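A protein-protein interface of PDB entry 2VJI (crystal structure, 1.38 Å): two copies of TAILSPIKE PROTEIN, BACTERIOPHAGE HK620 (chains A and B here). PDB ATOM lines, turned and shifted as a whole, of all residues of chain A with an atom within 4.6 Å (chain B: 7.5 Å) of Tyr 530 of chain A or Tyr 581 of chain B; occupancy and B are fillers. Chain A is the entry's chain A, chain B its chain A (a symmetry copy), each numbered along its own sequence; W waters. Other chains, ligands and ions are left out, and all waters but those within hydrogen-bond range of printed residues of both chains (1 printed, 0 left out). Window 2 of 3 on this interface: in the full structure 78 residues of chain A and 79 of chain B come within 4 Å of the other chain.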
ATOM      1  N   THR A 528      19.207   9.020 -26.433  1.00  0.00           N
ATOM      2  CA  THR A 528      20.408   8.218 -26.431  1.00  0.00           C
ATOM      3  C   THR A 528      20.297   7.299 -25.238  1.00  0.00           C
ATOM      4  O   THR A 528      19.520   7.536 -24.304  1.00  0.00           O
ATOM      5  CB  THR A 528      21.722   9.032 -26.364  1.00  0.00           C
ATOM      6  OG1 THR A 528      21.794   9.730 -25.119  1.00  0.00           O
ATOM      7  CG2 THR A 528      21.809   9.995 -27.534  1.00  0.00           C
ATOM      8  N   SER A 529      21.055   6.225 -25.285  1.00  0.00           N
ATOM      9  CA  SER A 529      21.124   5.278 -24.203  1.00  0.00           C
ATOM     10  C   SER A 529      22.492   5.156 -23.593  1.00  0.00           C
ATOM     11  O   SER A 529      23.478   5.602 -24.155  1.00  0.00           O
ATOM     12  CB  SER A 529      20.763   3.871 -24.677  1.00  0.00           C
ATOM     13  OG  SER A 529      21.824   3.220 -25.402  1.00  0.00           O
ATOM     14  N   TYR A 530      22.524   4.564 -22.403  1.00  0.00           N
ATOM     15  CA  TYR A 530      23.774   4.122 -21.848  1.00  0.00           C
ATOM     16  C   TYR A 530      24.278   2.896 -22.625  1.00  0.00           C
ATOM     17  O   TYR A 530      23.581   2.318 -23.482  1.00  0.00           O
ATOM     18  CB  TYR A 530      23.659   3.836 -20.360  1.00  0.00           C
ATOM     19  CG  TYR A 530      23.458   5.052 -19.466  1.00  0.00           C
ATOM     20  CD1 TYR A 530      23.771   6.355 -19.880  1.00  0.00           C
ATOM     21  CD2 TYR A 530      23.083   4.879 -18.145  1.00  0.00           C
ATOM     22  CE1 TYR A 530      23.625   7.455 -19.014  1.00  0.00           C
ATOM     23  CE2 TYR A 530      22.938   5.964 -17.296  1.00  0.00           C
ATOM     24  CZ  TYR A 530      23.216   7.234 -17.733  1.00  0.00           C
ATOM     25  OH  TYR A 530      23.087   8.343 -16.910  1.00  0.00           O
ATOM     26  N   ASN A 531      25.498   2.494 -22.301  1.00  0.00           N
ATOM     27  CA  ASN A 531      26.221   1.411 -22.993  1.00  0.00           C
ATOM     28  C   ASN A 531      25.872   0.000 -22.511  1.00  0.00           C
ATOM     29  O   ASN A 531      26.233  -0.998 -23.139  1.00  0.00           O
ATOM     30  CB  ASN A 531      27.710   1.673 -22.762  1.00  0.00           C
ATOM     31  CG  ASN A 531      28.619   0.755 -23.549  1.00  0.00           C
ATOM     32  OD1 ASN A 531      28.360   0.437 -24.706  1.00  0.00           O
ATOM     33  ND2 ASN A 531      29.729   0.371 -22.935  1.00  0.00           N
ATOM     34  N   THR A 532      25.210  -0.074 -21.366  1.00  0.00           N
ATOM     35  CA  THR A 532      24.835  -1.336 -20.711  1.00  0.00           C
ATOM     36  C   THR A 532      24.145  -2.392 -21.571  1.00  0.00           C
ATOM     37  O   THR A 532      23.173  -2.094 -22.217  1.00  0.00           O
ATOM     38  CB  THR A 532      23.885  -1.024 -19.515  1.00  0.00           C
ATOM     39  OG1 THR A 532      24.248   0.220 -18.904  1.00  0.00           O
ATOM     40  CG2 THR A 532      23.906  -2.135 -18.487  1.00  0.00           C
ATOM     41  N   VAL A 536      18.350  -1.186 -20.158  1.00  0.00           N
ATOM     42  CA  VAL A 536      19.198  -0.008 -20.226  1.00  0.00           C
ATOM     43  C   VAL A 536      18.352   1.231 -20.426  1.00  0.00           C
ATOM     44  O   VAL A 536      17.375   1.199 -21.157  1.00  0.00           O
ATOM     45  CB  VAL A 536      20.207  -0.165 -21.390  1.00  0.00           C
ATOM     46  CG1 VAL A 536      19.524  -0.222 -22.760  1.00  0.00           C
ATOM     47  CG2 VAL A 536      21.247   0.919 -21.378  1.00  0.00           C
ATOM     48  N   PRO A 537      18.697   2.325 -19.735  1.00  0.00           N
ATOM     49  CA  PRO A 537      17.912   3.540 -19.895  1.00  0.00           C
ATOM     50  C   PRO A 537      18.222   4.289 -21.186  1.00  0.00           C
ATOM     51  O   PRO A 537      19.365   4.298 -21.647  1.00  0.00           O
ATOM     52  CB  PRO A 537      18.324   4.370 -18.683  1.00  0.00           C
ATOM     53  CG  PRO A 537      19.770   3.981 -18.466  1.00  0.00           C
ATOM     54  CD  PRO A 537      19.751   2.491 -18.709  1.00  0.00           C
ATOM     55  N   PHE A 539      17.478   8.261 -22.649  1.00  0.00           N
ATOM     56  CA  PHE A 539      17.182   9.600 -22.141  1.00  0.00           C
ATOM     57  C   PHE A 539      17.089  10.561 -23.300  1.00  0.00           C
ATOM     58  O   PHE A 539      17.837  10.415 -24.262  1.00  0.00           O
ATOM     59  CB  PHE A 539      18.340  10.153 -21.298  1.00  0.00           C
ATOM     60  CG  PHE A 539      18.715   9.316 -20.120  1.00  0.00           C
ATOM     61  CD1 PHE A 539      19.661   8.310 -20.249  1.00  0.00           C
ATOM     62  CD2 PHE A 539      18.153   9.547 -18.882  1.00  0.00           C
ATOM     63  CE1 PHE A 539      20.028   7.550 -19.143  1.00  0.00           C
ATOM     64  CE2 PHE A 539      18.511   8.778 -17.769  1.00  0.00           C
ATOM     65  CZ  PHE A 539      19.458   7.793 -17.906  1.00  0.00           C
ATOM     66  N   VAL A 579      13.107   2.717 -19.807  1.00  0.00           N
ATOM     67  CA  VAL A 579      13.977   1.542 -19.815  1.00  0.00           C
ATOM     68  C   VAL A 579      13.735   0.723 -21.071  1.00  0.00           C
ATOM     69  O   VAL A 579      12.633   0.198 -21.313  1.00  0.00           O
ATOM     70  CB  VAL A 579      13.781   0.656 -18.548  1.00  0.00           C
ATOM     71  CG1 VAL A 579      14.633  -0.556 -18.612  1.00  0.00           C
ATOM     72  CG2 VAL A 579      14.115   1.463 -17.291  1.00  0.00           C
ATOM     73  N   ASN A 582      19.123  -3.563 -24.529  1.00  0.00           N
ATOM     74  CA  ASN A 582      20.281  -3.781 -25.403  1.00  0.00           C
ATOM     75  C   ASN A 582      20.563  -5.275 -25.465  1.00  0.00           C
ATOM     76  O   ASN A 582      21.051  -5.853 -24.483  1.00  0.00           O
ATOM     77  CB  ASN A 582      21.519  -3.077 -24.819  1.00  0.00           C
ATOM     78  CG  ASN A 582      21.914  -1.826 -25.555  1.00  0.00           C
ATOM     79  OD1 ASN A 582      21.579  -1.631 -26.737  1.00  0.00           O
ATOM     80  ND2 ASN A 582      22.724  -0.999 -24.891  1.00  0.00           N
ATOM     81  N   GLY A 586      26.206  -1.219 -26.140  1.00  0.00           N
ATOM     82  CA  GLY A 586      26.560  -0.103 -26.998  1.00  0.00           C
ATOM     83  C   GLY A 586      25.639   1.072 -26.762  1.00  0.00           C
ATOM     84  O   GLY A 586      24.470   0.898 -26.494  1.00  0.00           O
ATOM     85  N   VAL A 587      26.187   2.271 -26.848  1.00  0.00           N
ATOM     86  CA  VAL A 587      25.397   3.467 -26.794  1.00  0.00           C
ATOM     87  C   VAL A 587      24.536   3.525 -28.058  1.00  0.00           C
ATOM     88  O   VAL A 587      25.039   3.336 -29.183  1.00  0.00           O
ATOM     89  CB  VAL A 587      26.303   4.702 -26.732  1.00  0.00           C
ATOM     90  CG1 VAL A 587      25.527   5.968 -26.964  1.00  0.00           C
ATOM     91  CG2 VAL A 587      27.055   4.710 -25.432  1.00  0.00           C
ATOM     92  N   THR B 532      18.480  -1.920  -5.793  1.00  0.00           N
ATOM     93  CA  THR B 532      19.294  -2.102  -7.004  1.00  0.00           C
ATOM     94  C   THR B 532      19.614  -0.855  -7.825  1.00  0.00           C
ATOM     95  O   THR B 532      18.722  -0.125  -8.176  1.00  0.00           O
ATOM     96  CB  THR B 532      18.573  -3.106  -7.955  1.00  0.00           C
ATOM     97  OG1 THR B 532      17.881  -4.101  -7.193  1.00  0.00           O
ATOM     98  CG2 THR B 532      19.547  -3.762  -8.909  1.00  0.00           C
ATOM     99  N   GLN B 533      20.887  -0.664  -8.154  1.00  0.00           N
ATOM    100  CA  GLN B 533      21.272   0.379  -9.091  1.00  0.00           C
ATOM    101  C   GLN B 533      20.883  -0.144 -10.464  1.00  0.00           C
ATOM    102  O   GLN B 533      20.982  -1.343 -10.741  1.00  0.00           O
ATOM    103  CB  GLN B 533      22.775   0.664  -9.047  1.00  0.00           C
ATOM    104  CG  GLN B 533      23.245   1.858  -9.921  1.00  0.00           C
ATOM    105  CD  GLN B 533      23.316   1.586 -11.432  1.00  0.00           C
ATOM    106  OE1 GLN B 533      23.626   0.472 -11.889  1.00  0.00           O
ATOM    107  NE2 GLN B 533      23.036   2.616 -12.215  1.00  0.00           N
ATOM    108  N   GLY B 534      20.399   0.748 -11.302  1.00  0.00           N
ATOM    109  CA  GLY B 534      20.055   0.403 -12.684  1.00  0.00           C
ATOM    110  C   GLY B 534      18.571   0.155 -12.780  1.00  0.00           C
ATOM    111  O   GLY B 534      17.803   0.688 -11.997  1.00  0.00           O
ATOM    112  N   ALA B 535      18.152  -0.693 -13.708  1.00  0.00           N
ATOM    113  CA  ALA B 535      16.752  -1.017 -13.847  1.00  0.00           C
ATOM    114  C   ALA B 535      16.351  -1.693 -12.554  1.00  0.00           C
ATOM    115  O   ALA B 535      17.026  -2.619 -12.090  1.00  0.00           O
ATOM    116  CB  ALA B 535      16.555  -1.926 -15.017  1.00  0.00           C
ATOM    117  N   VAL B 536      15.223  -1.274 -12.017  1.00  0.00           N
ATOM    118  CA  VAL B 536      14.820  -1.719 -10.693  1.00  0.00           C
ATOM    119  C   VAL B 536      13.312  -1.695 -10.574  1.00  0.00           C
ATOM    120  O   VAL B 536      12.666  -0.793 -11.083  1.00  0.00           O
ATOM    121  CB  VAL B 536      15.460  -0.801  -9.622  1.00  0.00           C
ATOM    122  CG1 VAL B 536      14.958   0.643  -9.707  1.00  0.00           C
ATOM    123  CG2 VAL B 536      15.256  -1.337  -8.234  1.00  0.00           C
ATOM    124  N   PRO B 537      12.732  -2.722  -9.935  1.00  0.00           N
ATOM    125  CA  PRO B 537      11.284  -2.741  -9.797  1.00  0.00           C
ATOM    126  C   PRO B 537      10.772  -1.808  -8.705  1.00  0.00           C
ATOM    127  O   PRO B 537      11.429  -1.623  -7.679  1.00  0.00           O
ATOM    128  CB  PRO B 537      11.001  -4.196  -9.432  1.00  0.00           C
ATOM    129  CG  PRO B 537      12.217  -4.600  -8.628  1.00  0.00           C
ATOM    130  CD  PRO B 537      13.347  -3.954  -9.394  1.00  0.00           C
ATOM    131  N   PHE B 538       9.602  -1.221  -8.969  1.00  0.00           N
ATOM    132  CA  PHE B 538       8.817  -0.481  -7.982  1.00  0.00           C
ATOM    133  C   PHE B 538       7.527  -1.291  -7.796  1.00  0.00           C
ATOM    134  O   PHE B 538       6.937  -1.783  -8.766  1.00  0.00           O
ATOM    135  CB  PHE B 538       8.457   0.923  -8.443  1.00  0.00           C
ATOM    136  CG  PHE B 538       9.600   1.900  -8.430  1.00  0.00           C
ATOM    137  CD1 PHE B 538      10.701   1.728  -9.256  1.00  0.00           C
ATOM    138  CD2 PHE B 538       9.553   3.030  -7.618  1.00  0.00           C
ATOM    139  CE1 PHE B 538      11.752   2.663  -9.232  1.00  0.00           C
ATOM    140  CE2 PHE B 538      10.592   3.946  -7.607  1.00  0.00           C
ATOM    141  CZ  PHE B 538      11.678   3.763  -8.413  1.00  0.00           C
ATOM    142  N   ASN B 557       7.893  13.253 -12.414  1.00  0.00           N
ATOM    143  CA  ASN B 557       8.924  12.715 -11.551  1.00  0.00           C
ATOM    144  C   ASN B 557       9.921  13.832 -11.261  1.00  0.00           C
ATOM    145  O   ASN B 557      10.751  14.170 -12.129  1.00  0.00           O
ATOM    146  CB  ASN B 557       9.655  11.601 -12.250  1.00  0.00           C
ATOM    147  CG  ASN B 557      10.839  11.122 -11.461  1.00  0.00           C
ATOM    148  OD1 ASN B 557      10.733  10.956 -10.240  1.00  0.00           O
ATOM    149  ND2 ASN B 557      11.965  10.880 -12.129  1.00  0.00           N
ATOM    150  N   LEU B 560      16.164  13.465 -10.012  1.00  0.00           N
ATOM    151  CA  LEU B 560      17.227  13.246 -10.971  1.00  0.00           C
ATOM    152  C   LEU B 560      17.819  11.862 -10.815  1.00  0.00           C
ATOM    153  O   LEU B 560      18.154  11.204 -11.815  1.00  0.00           O
ATOM    154  CB  LEU B 560      18.389  14.235 -10.799  1.00  0.00           C
ATOM    155  CG  LEU B 560      18.354  15.629 -11.407  1.00  0.00           C
ATOM    156  CD1 LEU B 560      19.748  16.221 -11.291  1.00  0.00           C
ATOM    157  CD2 LEU B 560      17.928  15.595 -12.864  1.00  0.00           C
ATOM    158  N   ASP B 561      17.921  11.387  -9.579  1.00  0.00           N
ATOM    159  CA  ASP B 561      18.633  10.133  -9.298  1.00  0.00           C
ATOM    160  C   ASP B 561      17.893   8.856  -9.587  1.00  0.00           C
ATOM    161  O   ASP B 561      18.494   7.788  -9.549  1.00  0.00           O
ATOM    162  CB  ASP B 561      19.092  10.105  -7.841  1.00  0.00           C
ATOM    163  CG  ASP B 561      20.158  11.132  -7.536  1.00  0.00           C
ATOM    164  OD1 ASP B 561      20.703  11.768  -8.458  1.00  0.00           O
ATOM    165  OD2 ASP B 561      20.457  11.271  -6.340  1.00  0.00           O
ATOM    166  N   PHE B 562      16.602   8.949  -9.856  1.00  0.00           N
ATOM    167  CA  PHE B 562      15.827   7.780 -10.182  1.00  0.00           C
ATOM    168  C   PHE B 562      14.565   8.220 -10.898  1.00  0.00           C
ATOM    169  O   PHE B 562      14.191   9.409 -10.893  1.00  0.00           O
ATOM    170  CB  PHE B 562      15.460   6.970  -8.909  1.00  0.00           C
ATOM    171  CG  PHE B 562      14.395   7.597  -8.043  1.00  0.00           C
ATOM    172  CD1 PHE B 562      14.726   8.481  -7.043  1.00  0.00           C
ATOM    173  CD2 PHE B 562      13.056   7.271  -8.237  1.00  0.00           C
ATOM    174  CE1 PHE B 562      13.735   9.036  -6.246  1.00  0.00           C
ATOM    175  CE2 PHE B 562      12.073   7.837  -7.447  1.00  0.00           C
ATOM    176  CZ  PHE B 562      12.409   8.693  -6.463  1.00  0.00           C
ATOM    177  N   SER B 563      13.916   7.236 -11.507  1.00  0.00           N
ATOM    178  CA  SER B 563      12.633   7.447 -12.123  1.00  0.00           C
ATOM    179  C   SER B 563      11.789   6.207 -11.836  1.00  0.00           C
ATOM    180  O   SER B 563      12.290   5.092 -11.963  1.00  0.00           O
ATOM    181  CB  SER B 563      12.781   7.708 -13.618  1.00  0.00           C
ATOM    182  OG  SER B 563      13.514   6.667 -14.250  1.00  0.00           O
ATOM    183  N   PRO B 564      10.529   6.398 -11.415  1.00  0.00           N
ATOM    184  CA  PRO B 564       9.646   5.254 -11.270  1.00  0.00           C
ATOM    185  C   PRO B 564       9.217   4.808 -12.647  1.00  0.00           C
ATOM    186  O   PRO B 564       9.460   5.491 -13.628  1.00  0.00           O
ATOM    187  CB  PRO B 564       8.439   5.820 -10.523  1.00  0.00           C
ATOM    188  CG  PRO B 564       8.391   7.255 -10.971  1.00  0.00           C
ATOM    189  CD  PRO B 564       9.853   7.659 -11.052  1.00  0.00           C
ATOM    190  N   PRO B 565       8.550   3.668 -12.722  1.00  0.00           N
ATOM    191  CA  PRO B 565       8.098   3.190 -14.000  1.00  0.00           C
ATOM    192  C   PRO B 565       7.041   4.080 -14.644  1.00  0.00           C
ATOM    193  O   PRO B 565       6.269   4.664 -13.929  1.00  0.00           O
ATOM    194  CB  PRO B 565       7.412   1.872 -13.617  1.00  0.00           C
ATOM    195  CG  PRO B 565       7.901   1.521 -12.299  1.00  0.00           C
ATOM    196  CD  PRO B 565       8.152   2.778 -11.622  1.00  0.00           C
ATOM    197  N   GLY B 578       6.280  -2.359 -11.663  1.00  0.00           N
ATOM    198  CA  GLY B 578       6.805  -1.863 -12.917  1.00  0.00           C
ATOM    199  C   GLY B 578       8.302  -1.730 -12.801  1.00  0.00           C
ATOM    200  O   GLY B 578       8.853  -1.757 -11.716  1.00  0.00           O
ATOM    201  N   VAL B 579       8.967  -1.567 -13.923  1.00  0.00           N
ATOM    202  CA  VAL B 579      10.422  -1.418 -13.918  1.00  0.00           C
ATOM    203  C   VAL B 579      10.798   0.037 -14.133  1.00  0.00           C
ATOM    204  O   VAL B 579      10.506   0.646 -15.179  1.00  0.00           O
ATOM    205  CB  VAL B 579      11.108  -2.316 -14.991  1.00  0.00           C
ATOM    206  CG1 VAL B 579      12.575  -2.101 -15.002  1.00  0.00           C
ATOM    207  CG2 VAL B 579      10.799  -3.789 -14.714  1.00  0.00           C
ATOM    208  N   GLY B 580      11.450   0.586 -13.125  1.00  0.00           N
ATOM    209  CA  GLY B 580      11.957   1.957 -13.153  1.00  0.00           C
ATOM    210  C   GLY B 580      13.462   1.907 -13.252  1.00  0.00           C
ATOM    211  O   GLY B 580      14.045   0.893 -13.648  1.00  0.00           O
ATOM    212  N   TYR B 581      14.098   3.026 -12.922  1.00  0.00           N
ATOM    213  CA  TYR B 581      15.539   3.134 -13.043  1.00  0.00           C
ATOM    214  C   TYR B 581      16.160   3.922 -11.908  1.00  0.00           C
ATOM    215  O   TYR B 581      15.732   5.022 -11.628  1.00  0.00           O
ATOM    216  CB  TYR B 581      15.946   3.777 -14.399  1.00  0.00           C
ATOM    217  CG  TYR B 581      17.433   3.605 -14.695  1.00  0.00           C
ATOM    218  CD1 TYR B 581      17.927   2.386 -15.130  1.00  0.00           C
ATOM    219  CD2 TYR B 581      18.339   4.629 -14.491  1.00  0.00           C
ATOM    220  CE1 TYR B 581      19.279   2.191 -15.366  1.00  0.00           C
ATOM    221  CE2 TYR B 581      19.693   4.440 -14.724  1.00  0.00           C
ATOM    222  CZ  TYR B 581      20.155   3.208 -15.162  1.00  0.00           C
ATOM    223  OH  TYR B 581      21.504   2.991 -15.401  1.00  0.00           O
ATOM    224  N   ASN B 582      17.158   3.316 -11.277  1.00  0.00           N
ATOM    225  CA  ASN B 582      17.964   3.947 -10.226  1.00  0.00           C
ATOM    226  C   ASN B 582      19.299   4.360 -10.827  1.00  0.00           C
ATOM    227  O   ASN B 582      20.142   3.498 -11.113  1.00  0.00           O
ATOM    228  CB  ASN B 582      18.233   2.939  -9.094  1.00  0.00           C
ATOM    229  CG  ASN B 582      17.432   3.196  -7.846  1.00  0.00           C
ATOM    230  OD1 ASN B 582      16.964   4.319  -7.591  1.00  0.00           O
ATOM    231  ND2 ASN B 582      17.346   2.170  -6.997  1.00  0.00           N
ATOM    232  N   GLU B 583      19.528   5.659 -11.016  1.00  0.00           N
ATOM    233  CA  GLU B 583      20.830   6.132 -11.539  1.00  0.00           C
ATOM    234  C   GLU B 583      21.892   5.754 -10.513  1.00  0.00           C
ATOM    235  O   GLU B 583      22.993   5.335 -10.841  1.00  0.00           O
ATOM    236  CB  GLU B 583      20.850   7.648 -11.750  1.00  0.00           C
ATOM    237  CG  GLU B 583      22.139   8.242 -12.339  1.00  0.00           C
ATOM    238  CD  GLU B 583      22.284   8.041 -13.841  1.00  0.00           C
ATOM    239  OE1 GLU B 583      21.293   7.683 -14.510  1.00  0.00           O
ATOM    240  OE2 GLU B 583      23.396   8.286 -14.356  1.00  0.00           O
ATOM    241  N   ILE B 584      21.524   5.957  -9.250  1.00  0.00           N
ATOM    242  CA  ILE B 584      22.297   5.606  -8.095  1.00  0.00           C
ATOM    243  C   ILE B 584      21.393   4.665  -7.320  1.00  0.00           C
ATOM    244  O   ILE B 584      20.177   4.813  -7.375  1.00  0.00           O
ATOM    245  CB  ILE B 584      22.574   6.903  -7.270  1.00  0.00           C
ATOM    246  CG1 ILE B 584      23.510   7.833  -8.053  1.00  0.00           C
ATOM    247  CG2 ILE B 584      23.100   6.596  -5.891  1.00  0.00           C
ATOM    248  CD1 ILE B 584      24.738   7.166  -8.561  1.00  0.00           C
ATOM    249  N   ARG B 588      13.653   3.518  -2.898  1.00  0.00           N
ATOM    250  CA  ARG B 588      12.862   4.713  -3.199  1.00  0.00           C
ATOM    251  C   ARG B 588      11.447   4.538  -2.742  1.00  0.00           C
ATOM    252  O   ARG B 588      10.955   3.427  -2.657  1.00  0.00           O
ATOM    253  CB  ARG B 588      12.858   4.976  -4.696  1.00  0.00           C
ATOM    254  CG  ARG B 588      14.210   4.961  -5.341  1.00  0.00           C
ATOM    255  CD  ARG B 588      15.149   5.961  -4.708  1.00  0.00           C
ATOM    256  NE  ARG B 588      16.417   5.974  -5.421  1.00  0.00           N
ATOM    257  CZ  ARG B 588      17.365   6.864  -5.233  1.00  0.00           C
ATOM    258  NH1 ARG B 588      17.211   7.840  -4.347  1.00  0.00           N
ATOM    259  NH2 ARG B 588      18.478   6.766  -5.939  1.00  0.00           N
HETATM  260  O   HOH W   1      22.295   0.901 -16.798  1.00  0.00           O
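The side-chain carboxylate (OE2) of Glu 583 of chain B sits at hydrogen-bond distance from the side-chain hydroxyl (OH) of Tyr 530 of chain A, at 2.6 Å.
The backbone NH (N) of Phe 539 of chain A lies within hydrogen-bond range of the backbone carbonyl oxygen (O) of Thr 528 of chain A, 2.7 Å away.
The backbone NH of Tyr 530 of chain A sits at hydrogen-bond distance from the backbone carbonyl oxygen of Pro 537 of chain A (3.3 Å).
The side-chain amide nitrogen (NE2) of Gln 533 of chain B is in hydrogen-bond range of the backbone carbonyl oxygen (O) of Glu 583 of chain B, 3.0 Å away.
N of Gly 580 of chain B is in hydrogen-bond range of O of Val 536 of chain B.
The backbone carbonyl oxygen of Asp 561 of chain B sits at hydrogen-bond distance from the backbone NH of Glu 583 of chain B, at 2.8 Å.
The backbone NH (N) of Ser 563 of chain B lies within hydrogen-bond range of the backbone carbonyl oxygen (O) of Tyr 581 of chain B, 2.9 Å away.
Tyr 530 of chain A touches Tyr 581 of chain B (CD2 to OH, 3.7 Å).
Pro 537 of chain A touches Tyr 581 of chain B.
Glu 583 of chain B touches Phe 539 of chain A.
CG2 of Val 579 of chain A touches O of Gly 580 of chain B, at 3.7 Å.
Of the printed residues of chain B, Phe 539 of chain A touches Glu 583 (3.9 Å).
Of the printed residues of chain B, Val 579 of chain A touches Gly 580.
Gly 586 of chain A touches none of the printed residues of chain B.
Asp 561 of chain B touches none of the printed residues of chain A.
Of chain A, only Tyr 530 and Pro 537 come within 4 Å of Tyr 581 of chain B.
Hydrophobic or aromatic side chains of chain B that line the printed part of chain A: Tyr 581.
Along chain B the printed residues that touch a printed residue of chain A span positions 580 to 583.
Of the 12 printed residues of chain A, 4 touch a printed residue of chain B.
Among the printed residues, 5 pairs touch across the chains.
Among the printed residues, no Asp or Glu carboxylate lies within 4 Å of a Lys or Arg side-chain nitrogen of the other chain.
Positions printed for both chains: 532, 536, 537, 579 and 582.
Of the 5 pairs that touch across the chains among the printed residues, none has its exchanged pair printed and touching as well.
Water W1 bridges the side-chain hydroxyl (OH) of Tyr 581 of chain B and the side-chain hydroxyl (OG1) of Thr 532 of chain A.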
